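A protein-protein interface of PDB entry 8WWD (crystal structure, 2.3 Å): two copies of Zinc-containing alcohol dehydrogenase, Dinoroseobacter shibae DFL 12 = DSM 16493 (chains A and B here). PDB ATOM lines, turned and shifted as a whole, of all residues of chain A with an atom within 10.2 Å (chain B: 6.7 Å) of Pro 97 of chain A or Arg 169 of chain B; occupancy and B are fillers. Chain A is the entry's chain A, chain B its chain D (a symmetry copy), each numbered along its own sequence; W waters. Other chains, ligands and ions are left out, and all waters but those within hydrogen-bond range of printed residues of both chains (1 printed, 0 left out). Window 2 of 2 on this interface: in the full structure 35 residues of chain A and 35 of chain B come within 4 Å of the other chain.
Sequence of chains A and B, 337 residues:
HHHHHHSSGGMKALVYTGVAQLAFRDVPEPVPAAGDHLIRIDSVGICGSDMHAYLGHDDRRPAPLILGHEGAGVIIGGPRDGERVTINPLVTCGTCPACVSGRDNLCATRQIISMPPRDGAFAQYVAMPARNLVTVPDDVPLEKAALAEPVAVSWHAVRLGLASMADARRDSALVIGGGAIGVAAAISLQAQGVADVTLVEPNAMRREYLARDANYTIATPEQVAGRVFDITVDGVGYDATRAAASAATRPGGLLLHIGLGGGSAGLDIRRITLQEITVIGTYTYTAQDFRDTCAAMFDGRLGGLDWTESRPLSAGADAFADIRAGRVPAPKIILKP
Among the printed residues, merely in contact across the chains: Pro 97 of chain A with Arg 169 of chain B (3.9 Å), Ala 98 of chain A with Arg 169 of chain B (3.9 Å), Ser 101 of chain A with Asp 167 of chain B (3.5 Å), Leu 106 of chain A with Pro 251 of chain B (3.9 Å) and Leu 106 of chain A with Gly 252 of chain B (3.5 Å).
The backbone NH (N) of Ala 98 of chain A sits close to the side-chain sulfur (SG) of Cys 96 of chain A (3.7 Å).
O of Ala 98 of chain A is in hydrogen-bond range of N of Arg 103 of chain A, at 2.9 Å.
O of Arg 103 of chain A sits close to OD1 of Asn 105 of chain A (3.0 Å).
The side-chain carboxylate (OD1) of Asp 167 of chain B is in hydrogen-bond range of the backbone NH (N) of Arg 169 of chain B (3.1 Å).
The guanidinium group (NH1) of Arg 250 of chain B is in salt-bridge range of the side-chain carboxylate (OD1) of Asp 167 of chain B, at 2.5 Å.
The backbone carbonyl oxygen (O) of Arg 169 of chain B lies within hydrogen-bond range of the guanidinium group (NH1) of Arg 250 of chain B (3.1 Å).
No position is printed for both chains.
Of the 7 pairs that touch across the chains among the printed residues, none has its exchanged pair printed and touching as well.
The guanidinium group (NH1) of Arg 103 of chain A lies within salt-bridge range of the side-chain carboxylate (OD2) of Asp 167 of chain B (3.0 Å).
The guanidinium group of Arg 103 of chain A sits at hydrogen-bond distance from the backbone carbonyl oxygen of Gly 252 of chain B, 2.7 Å away.
Hydrophobic or aromatic side chains of chain A within 4 Å of the printed part of chain B: Pro 97 and Leu 106.
Among the printed residues, 7 pairs touch across the chains.
Among the printed residues, Asp or Glu carboxylates within 4 Å of a Lys or Arg side-chain nitrogen of the other chain: Arg 103 of chain A with Asp 167 of chain B.
Pro 97 of chain A touches just one residue of chain B: Arg 169 (3.9 Å).
Of the printed residues of chain B, Ala 98 of chain A touches Arg 169 (3.9 Å).
Cys 99 of chain A touches none of the printed residues of chain B.
Printed residues of chain B within 4 Å of Ser 101 of chain A: Asp 167.
No residue of chain A comes within 4 Å of Ala 168 of chain B.
Of the printed residues of chain A, Arg 169 of chain B touches Pro 97 and Ala 98.
Asp 230 of chain B touches none of the printed residues of chain A.
The nearest printed residue of chain B that does not touch Pro 97 of chain A is Asp 167 of chain B (6.7 Å).
Water W1 lies within hydrogen-bond range of OG of Ser 101 of chain A (2.6 Å), OD2 of Asp 167 of chain B (2.8 Å) and NH1 of Arg 169 of chain B (3.0 Å).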
ATOM      1  N   CYS A  93     -11.477  18.882   7.678  1.00  0.00           N
ATOM      2  CA  CYS A  93     -12.435  19.621   8.551  1.00  0.00           C
ATOM      3  C   CYS A  93     -12.451  19.005   9.966  1.00  0.00           C
ATOM      4  O   CYS A  93     -12.790  19.730  10.931  1.00  0.00           O
ATOM      5  CB  CYS A  93     -13.815  19.661   7.898  1.00  0.00           C
ATOM      6  SG  CYS A  93     -14.786  18.208   8.175  1.00  0.00           S
ATOM      7  N   GLY A  94     -12.171  17.708  10.098  1.00  0.00           N
ATOM      8  CA  GLY A  94     -12.194  16.987  11.386  1.00  0.00           C
ATOM      9  C   GLY A  94     -13.587  16.584  11.886  1.00  0.00           C
ATOM     10  O   GLY A  94     -13.627  15.846  12.901  1.00  0.00           O
ATOM     11  N   THR A  95     -14.697  16.991  11.246  1.00  0.00           N
ATOM     12  CA  THR A  95     -16.078  16.731  11.771  1.00  0.00           C
ATOM     13  C   THR A  95     -17.033  16.097  10.754  1.00  0.00           C
ATOM     14  O   THR A  95     -18.170  15.829  11.176  1.00  0.00           O
ATOM     15  CB  THR A  95     -16.753  18.003  12.294  1.00  0.00           C
ATOM     16  OG1 THR A  95     -16.903  18.894  11.191  1.00  0.00           O
ATOM     17  CG2 THR A  95     -15.952  18.678  13.382  1.00  0.00           C
ATOM     18  N   CYS A  96     -16.624  15.847   9.505  1.00  0.00           N
ATOM     19  CA  CYS A  96     -17.465  15.176   8.484  1.00  0.00           C
ATOM     20  C   CYS A  96     -17.448  13.661   8.728  1.00  0.00           C
ATOM     21  O   CYS A  96     -16.651  13.142   9.504  1.00  0.00           O
ATOM     22  CB  CYS A  96     -17.015  15.561   7.080  1.00  0.00           C
ATOM     23  SG  CYS A  96     -15.516  14.807   6.531  1.00  0.00           S
ATOM     24  N   PRO A  97     -18.351  12.879   8.112  1.00  0.00           N
ATOM     25  CA  PRO A  97     -18.334  11.423   8.289  1.00  0.00           C
ATOM     26  C   PRO A  97     -16.998  10.745   7.943  1.00  0.00           C
ATOM     27  O   PRO A  97     -16.584   9.788   8.590  1.00  0.00           O
ATOM     28  CB  PRO A  97     -19.443  10.956   7.333  1.00  0.00           C
ATOM     29  CG  PRO A  97     -20.398  12.145   7.287  1.00  0.00           C
ATOM     30  CD  PRO A  97     -19.470  13.346   7.277  1.00  0.00           C
ATOM     31  N   ALA A  98     -16.337  11.190   6.884  1.00  0.00           N
ATOM     32  CA  ALA A  98     -15.034  10.590   6.532  1.00  0.00           C
ATOM     33  C   ALA A  98     -14.038  10.884   7.671  1.00  0.00           C
ATOM     34  O   ALA A  98     -13.349   9.974   8.100  1.00  0.00           O
ATOM     35  CB  ALA A  98     -14.591  11.066   5.175  1.00  0.00           C
ATOM     36  N   CYS A  99     -14.007  12.111   8.189  1.00  0.00           N
ATOM     37  CA  CYS A  99     -13.035  12.531   9.230  1.00  0.00           C
ATOM     38  C   CYS A  99     -13.350  11.758  10.516  1.00  0.00           C
ATOM     39  O   CYS A  99     -12.421  11.171  11.101  1.00  0.00           O
ATOM     40  CB  CYS A  99     -13.050  14.046   9.433  1.00  0.00           C
ATOM     41  SG  CYS A  99     -12.333  14.959   8.067  1.00  0.00           S
ATOM     42  N   VAL A 100     -14.622  11.709  10.912  1.00  0.00           N
ATOM     43  CA  VAL A 100     -15.069  11.020  12.160  1.00  0.00           C
ATOM     44  C   VAL A 100     -14.682   9.537  12.057  1.00  0.00           C
ATOM     45  O   VAL A 100     -14.293   8.964  13.071  1.00  0.00           O
ATOM     46  CB  VAL A 100     -16.583  11.218  12.395  1.00  0.00           C
ATOM     47  CG1 VAL A 100     -17.173  10.155  13.311  1.00  0.00           C
ATOM     48  CG2 VAL A 100     -16.882  12.616  12.920  1.00  0.00           C
ATOM     49  N   SER A 101     -14.786   8.968  10.856  1.00  0.00           N
ATOM     50  CA  SER A 101     -14.394   7.586  10.474  1.00  0.00           C
ATOM     51  C   SER A 101     -12.869   7.342  10.577  1.00  0.00           C
ATOM     52  O   SER A 101     -12.457   6.168  10.541  1.00  0.00           O
ATOM     53  CB  SER A 101     -14.869   7.331   9.066  1.00  0.00           C
ATOM     54  OG  SER A 101     -14.194   6.231   8.497  1.00  0.00           O
ATOM     55  N   GLY A 102     -12.040   8.387  10.665  1.00  0.00           N
ATOM     56  CA  GLY A 102     -10.569   8.249  10.661  1.00  0.00           C
ATOM     57  C   GLY A 102      -9.974   8.290   9.253  1.00  0.00           C
ATOM     58  O   GLY A 102      -8.748   8.093   9.123  1.00  0.00           O
ATOM     59  N   ARG A 103     -10.792   8.566   8.234  1.00  0.00           N
ATOM     60  CA  ARG A 103     -10.382   8.600   6.810  1.00  0.00           C
ATOM     61  C   ARG A 103     -10.399  10.062   6.336  1.00  0.00           C
ATOM     62  O   ARG A 103     -10.945  10.364   5.249  1.00  0.00           O
ATOM     63  CB  ARG A 103     -11.285   7.661   6.006  1.00  0.00           C
ATOM     64  CG  ARG A 103     -11.133   6.203   6.418  1.00  0.00           C
ATOM     65  CD  ARG A 103     -11.859   5.267   5.471  1.00  0.00           C
ATOM     66  NE  ARG A 103     -11.176   5.040   4.210  1.00  0.00           N
ATOM     67  CZ  ARG A 103     -11.681   4.330   3.199  1.00  0.00           C
ATOM     68  NH1 ARG A 103     -12.861   3.736   3.326  1.00  0.00           N
ATOM     69  NH2 ARG A 103     -10.995   4.192   2.078  1.00  0.00           N
ATOM     70  N   ASP A 104      -9.749  10.937   7.099  1.00  0.00           N
ATOM     71  CA  ASP A 104      -9.754  12.401   6.849  1.00  0.00           C
ATOM     72  C   ASP A 104      -9.146  12.725   5.479  1.00  0.00           C
ATOM     73  O   ASP A 104      -9.452  13.808   4.971  1.00  0.00           O
ATOM     74  CB  ASP A 104      -9.074  13.115   8.006  1.00  0.00           C
ATOM     75  CG  ASP A 104      -7.764  12.460   8.382  1.00  0.00           C
ATOM     76  OD1 ASP A 104      -6.795  12.671   7.630  1.00  0.00           O
ATOM     77  OD2 ASP A 104      -7.743  11.727   9.413  1.00  0.00           O
ATOM     78  N   ASN A 105      -8.365  11.823   4.869  1.00  0.00           N
ATOM     79  CA  ASN A 105      -7.925  11.940   3.449  1.00  0.00           C
ATOM     80  C   ASN A 105      -9.133  12.057   2.504  1.00  0.00           C
ATOM     81  O   ASN A 105      -8.947  12.558   1.396  1.00  0.00           O
ATOM     82  CB  ASN A 105      -7.063  10.764   3.006  1.00  0.00           C
ATOM     83  CG  ASN A 105      -7.791   9.433   3.068  1.00  0.00           C
ATOM     84  OD1 ASN A 105      -8.527   9.168   4.018  1.00  0.00           O
ATOM     85  ND2 ASN A 105      -7.595   8.590   2.063  1.00  0.00           N
ATOM     86  N   LEU A 106     -10.317  11.595   2.922  1.00  0.00           N
ATOM     87  CA  LEU A 106     -11.582  11.639   2.146  1.00  0.00           C
ATOM     88  C   LEU A 106     -12.526  12.715   2.689  1.00  0.00           C
ATOM     89  O   LEU A 106     -13.710  12.680   2.330  1.00  0.00           O
ATOM     90  CB  LEU A 106     -12.241  10.261   2.221  1.00  0.00           C
ATOM     91  CG  LEU A 106     -11.371   9.129   1.696  1.00  0.00           C
ATOM     92  CD1 LEU A 106     -12.110   7.804   1.775  1.00  0.00           C
ATOM     93  CD2 LEU A 106     -10.902   9.421   0.278  1.00  0.00           C
ATOM     94  N   CYS A 107     -12.014  13.664   3.475  1.00  0.00           N
ATOM     95  CA  CYS A 107     -12.793  14.801   4.010  1.00  0.00           C
ATOM     96  C   CYS A 107     -13.585  15.461   2.876  1.00  0.00           C
ATOM     97  O   CYS A 107     -12.988  15.795   1.834  1.00  0.00           O
ATOM     98  CB  CYS A 107     -11.895  15.834   4.675  1.00  0.00           C
ATOM     99  SG  CYS A 107     -12.830  17.285   5.109  1.00  0.00           S
ATOM    100  N   ALA A 108     -14.876  15.699   3.097  1.00  0.00           N
ATOM    101  CA  ALA A 108     -15.794  16.254   2.077  1.00  0.00           C
ATOM    102  C   ALA A 108     -15.377  17.685   1.706  1.00  0.00           C
ATOM    103  O   ALA A 108     -15.728  18.098   0.611  1.00  0.00           O
ATOM    104  CB  ALA A 108     -17.230  16.193   2.563  1.00  0.00           C
ATOM    105  N   THR A 109     -14.662  18.424   2.568  1.00  0.00           N
ATOM    106  CA  THR A 109     -14.203  19.805   2.235  1.00  0.00           C
ATOM    107  C   THR A 109     -12.668  19.881   2.235  1.00  0.00           C
ATOM    108  O   THR A 109     -12.129  20.965   2.412  1.00  0.00           O
ATOM    109  CB  THR A 109     -14.860  20.841   3.148  1.00  0.00           C
ATOM    110  OG1 THR A 109     -14.520  20.481   4.483  1.00  0.00           O
ATOM    111  CG2 THR A 109     -16.363  20.885   2.996  1.00  0.00           C
ATOM    112  N   MET B 165     -13.969  -3.908   3.496  1.00  0.00           N
ATOM    113  CA  MET B 165     -14.221  -2.446   3.530  1.00  0.00           C
ATOM    114  C   MET B 165     -13.285  -1.807   4.554  1.00  0.00           C
ATOM    115  O   MET B 165     -13.057  -2.411   5.626  1.00  0.00           O
ATOM    116  CB  MET B 165     -15.673  -2.105   3.882  1.00  0.00           C
ATOM    117  CG  MET B 165     -16.605  -2.210   2.684  1.00  0.00           C
ATOM    118  SD  MET B 165     -18.328  -2.002   3.158  1.00  0.00           S
ATOM    119  CE  MET B 165     -18.408  -0.273   3.608  1.00  0.00           C
ATOM    120  N   ASP B 167     -13.747   0.897   6.296  1.00  0.00           N
ATOM    121  CA  ASP B 167     -14.478   1.582   7.395  1.00  0.00           C
ATOM    122  C   ASP B 167     -15.773   0.814   7.695  1.00  0.00           C
ATOM    123  O   ASP B 167     -16.100  -0.100   6.933  1.00  0.00           O
ATOM    124  CB  ASP B 167     -14.716   3.064   7.082  1.00  0.00           C
ATOM    125  CG  ASP B 167     -15.587   3.361   5.872  1.00  0.00           C
ATOM    126  OD1 ASP B 167     -16.647   2.714   5.762  1.00  0.00           O
ATOM    127  OD2 ASP B 167     -15.213   4.268   5.058  1.00  0.00           O
ATOM    128  N   ALA B 168     -16.480   1.206   8.762  1.00  0.00           N
ATOM    129  CA  ALA B 168     -17.659   0.506   9.326  1.00  0.00           C
ATOM    130  C   ALA B 168     -18.960   1.170   8.870  1.00  0.00           C
ATOM    131  O   ALA B 168     -20.001   0.886   9.507  1.00  0.00           O
ATOM    132  CB  ALA B 168     -17.575   0.500  10.834  1.00  0.00           C
ATOM    133  N   ARG B 169     -18.909   2.015   7.835  1.00  0.00           N
ATOM    134  CA  ARG B 169     -20.082   2.783   7.348  1.00  0.00           C
ATOM    135  C   ARG B 169     -20.749   1.961   6.253  1.00  0.00           C
ATOM    136  O   ARG B 169     -20.276   1.994   5.108  1.00  0.00           O
ATOM    137  CB  ARG B 169     -19.692   4.182   6.870  1.00  0.00           C
ATOM    138  CG  ARG B 169     -19.159   5.081   7.978  1.00  0.00           C
ATOM    139  CD  ARG B 169     -18.506   6.326   7.412  1.00  0.00           C
ATOM    140  NE  ARG B 169     -19.384   6.936   6.424  1.00  0.00           N
ATOM    141  CZ  ARG B 169     -18.984   7.660   5.391  1.00  0.00           C
ATOM    142  NH1 ARG B 169     -17.696   7.905   5.191  1.00  0.00           N
ATOM    143  NH2 ARG B 169     -19.885   8.140   4.550  1.00  0.00           N
ATOM    144  N   ARG B 170     -21.833   1.291   6.632  1.00  0.00           N
ATOM    145  CA  ARG B 170     -22.480   0.185   5.888  1.00  0.00           C
ATOM    146  C   ARG B 170     -23.978   0.458   5.746  1.00  0.00           C
ATOM    147  O   ARG B 170     -24.744  -0.511   5.737  1.00  0.00           O
ATOM    148  CB  ARG B 170     -22.267  -1.082   6.711  1.00  0.00           C
ATOM    149  CG  ARG B 170     -22.419  -2.370   5.926  1.00  0.00           C
ATOM    150  CD  ARG B 170     -22.011  -3.536   6.797  1.00  0.00           C
ATOM    151  NE  ARG B 170     -20.638  -3.374   7.248  1.00  0.00           N
ATOM    152  CZ  ARG B 170     -19.933  -4.305   7.862  1.00  0.00           C
ATOM    153  NH1 ARG B 170     -20.459  -5.492   8.115  1.00  0.00           N
ATOM    154  NH2 ARG B 170     -18.694  -4.041   8.227  1.00  0.00           N
ATOM    155  N   ASP B 171     -24.376   1.728   5.672  1.00  0.00           N
ATOM    156  CA  ASP B 171     -25.797   2.160   5.762  1.00  0.00           C
ATOM    157  C   ASP B 171     -26.527   1.817   4.459  1.00  0.00           C
ATOM    158  O   ASP B 171     -27.632   1.255   4.553  1.00  0.00           O
ATOM    159  CB  ASP B 171     -25.903   3.644   6.116  1.00  0.00           C
ATOM    160  CG  ASP B 171     -25.299   3.968   7.468  1.00  0.00           C
ATOM    161  OD1 ASP B 171     -25.161   3.042   8.295  1.00  0.00           O
ATOM    162  OD2 ASP B 171     -24.931   5.135   7.667  1.00  0.00           O
ATOM    163  N   SER B 172     -25.916   2.092   3.304  1.00  0.00           N
ATOM    164  CA  SER B 172     -26.588   2.120   1.974  1.00  0.00           C
ATOM    165  C   SER B 172     -25.961   1.108   1.016  1.00  0.00           C
ATOM    166  O   SER B 172     -24.724   1.119   0.867  1.00  0.00           O
ATOM    167  CB  SER B 172     -26.501   3.493   1.369  1.00  0.00           C
ATOM    168  OG  SER B 172     -27.317   4.385   2.080  1.00  0.00           O
ATOM    169  N   ASP B 230     -22.859   3.492   0.294  1.00  0.00           N
ATOM    170  CA  ASP B 230     -21.677   2.880   0.941  1.00  0.00           C
ATOM    171  C   ASP B 230     -21.207   1.699   0.091  1.00  0.00           C
ATOM    172  O   ASP B 230     -19.968   1.546  -0.070  1.00  0.00           O
ATOM    173  CB  ASP B 230     -21.993   2.468   2.376  1.00  0.00           C
ATOM    174  CG  ASP B 230     -22.437   3.630   3.244  1.00  0.00           C
ATOM    175  OD1 ASP B 230     -21.694   4.624   3.310  1.00  0.00           O
ATOM    176  OD2 ASP B 230     -23.526   3.538   3.826  1.00  0.00           O
ATOM    177  N   ILE B 231     -22.156   0.916  -0.441  1.00  0.00           N
ATOM    178  CA  ILE B 231     -21.894  -0.357  -1.185  1.00  0.00           C
ATOM    179  C   ILE B 231     -22.624  -0.335  -2.519  1.00  0.00           C
ATOM    180  O   ILE B 231     -23.817   0.001  -2.520  1.00  0.00           O
ATOM    181  CB  ILE B 231     -22.345  -1.570  -0.358  1.00  0.00           C
ATOM    182  CG1 ILE B 231     -21.814  -1.465   1.073  1.00  0.00           C
ATOM    183  CG2 ILE B 231     -21.930  -2.858  -1.050  1.00  0.00           C
ATOM    184  CD1 ILE B 231     -22.281  -2.563   2.005  1.00  0.00           C
ATOM    185  N   ARG B 250     -19.871   5.910  -2.861  1.00  0.00           N
ATOM    186  CA  ARG B 250     -19.402   7.023  -1.999  1.00  0.00           C
ATOM    187  C   ARG B 250     -17.892   6.910  -1.847  1.00  0.00           C
ATOM    188  O   ARG B 250     -17.362   5.807  -1.936  1.00  0.00           O
ATOM    189  CB  ARG B 250     -20.080   6.968  -0.628  1.00  0.00           C
ATOM    190  CG  ARG B 250     -19.580   5.837   0.261  1.00  0.00           C
ATOM    191  CD  ARG B 250     -19.595   6.148   1.745  1.00  0.00           C
ATOM    192  NE  ARG B 250     -19.279   4.965   2.543  1.00  0.00           N
ATOM    193  CZ  ARG B 250     -18.091   4.653   3.069  1.00  0.00           C
ATOM    194  NH1 ARG B 250     -17.964   3.537   3.771  1.00  0.00           N
ATOM    195  NH2 ARG B 250     -17.040   5.444   2.910  1.00  0.00           N
ATOM    196  N   PRO B 251     -17.169   8.032  -1.617  1.00  0.00           N
ATOM    197  CA  PRO B 251     -15.717   7.991  -1.413  1.00  0.00           C
ATOM    198  C   PRO B 251     -15.348   7.073  -0.232  1.00  0.00           C
ATOM    199  O   PRO B 251     -15.973   7.176   0.831  1.00  0.00           O
ATOM    200  CB  PRO B 251     -15.341   9.450  -1.111  1.00  0.00           C
ATOM    201  CG  PRO B 251     -16.491  10.280  -1.668  1.00  0.00           C
ATOM    202  CD  PRO B 251     -17.716   9.399  -1.549  1.00  0.00           C
ATOM    203  N   GLY B 252     -14.397   6.160  -0.440  1.00  0.00           N
ATOM    204  CA  GLY B 252     -14.011   5.161   0.575  1.00  0.00           C
ATOM    205  C   GLY B 252     -14.914   3.929   0.558  1.00  0.00           C
ATOM    206  O   GLY B 252     -14.759   3.071   1.477  1.00  0.00           O
ATOM    207  N   GLY B 253     -15.811   3.836  -0.438  1.00  0.00           N
ATOM    208  CA  GLY B 253     -16.895   2.843  -0.490  1.00  0.00           C
ATOM    209  C   GLY B 253     -16.468   1.572  -1.185  1.00  0.00           C
ATOM    210  O   GLY B 253     -15.280   1.477  -1.616  1.00  0.00           O
HETATM  211  O   HOH W   1     -14.999   6.877   6.136  1.00  0.00           O
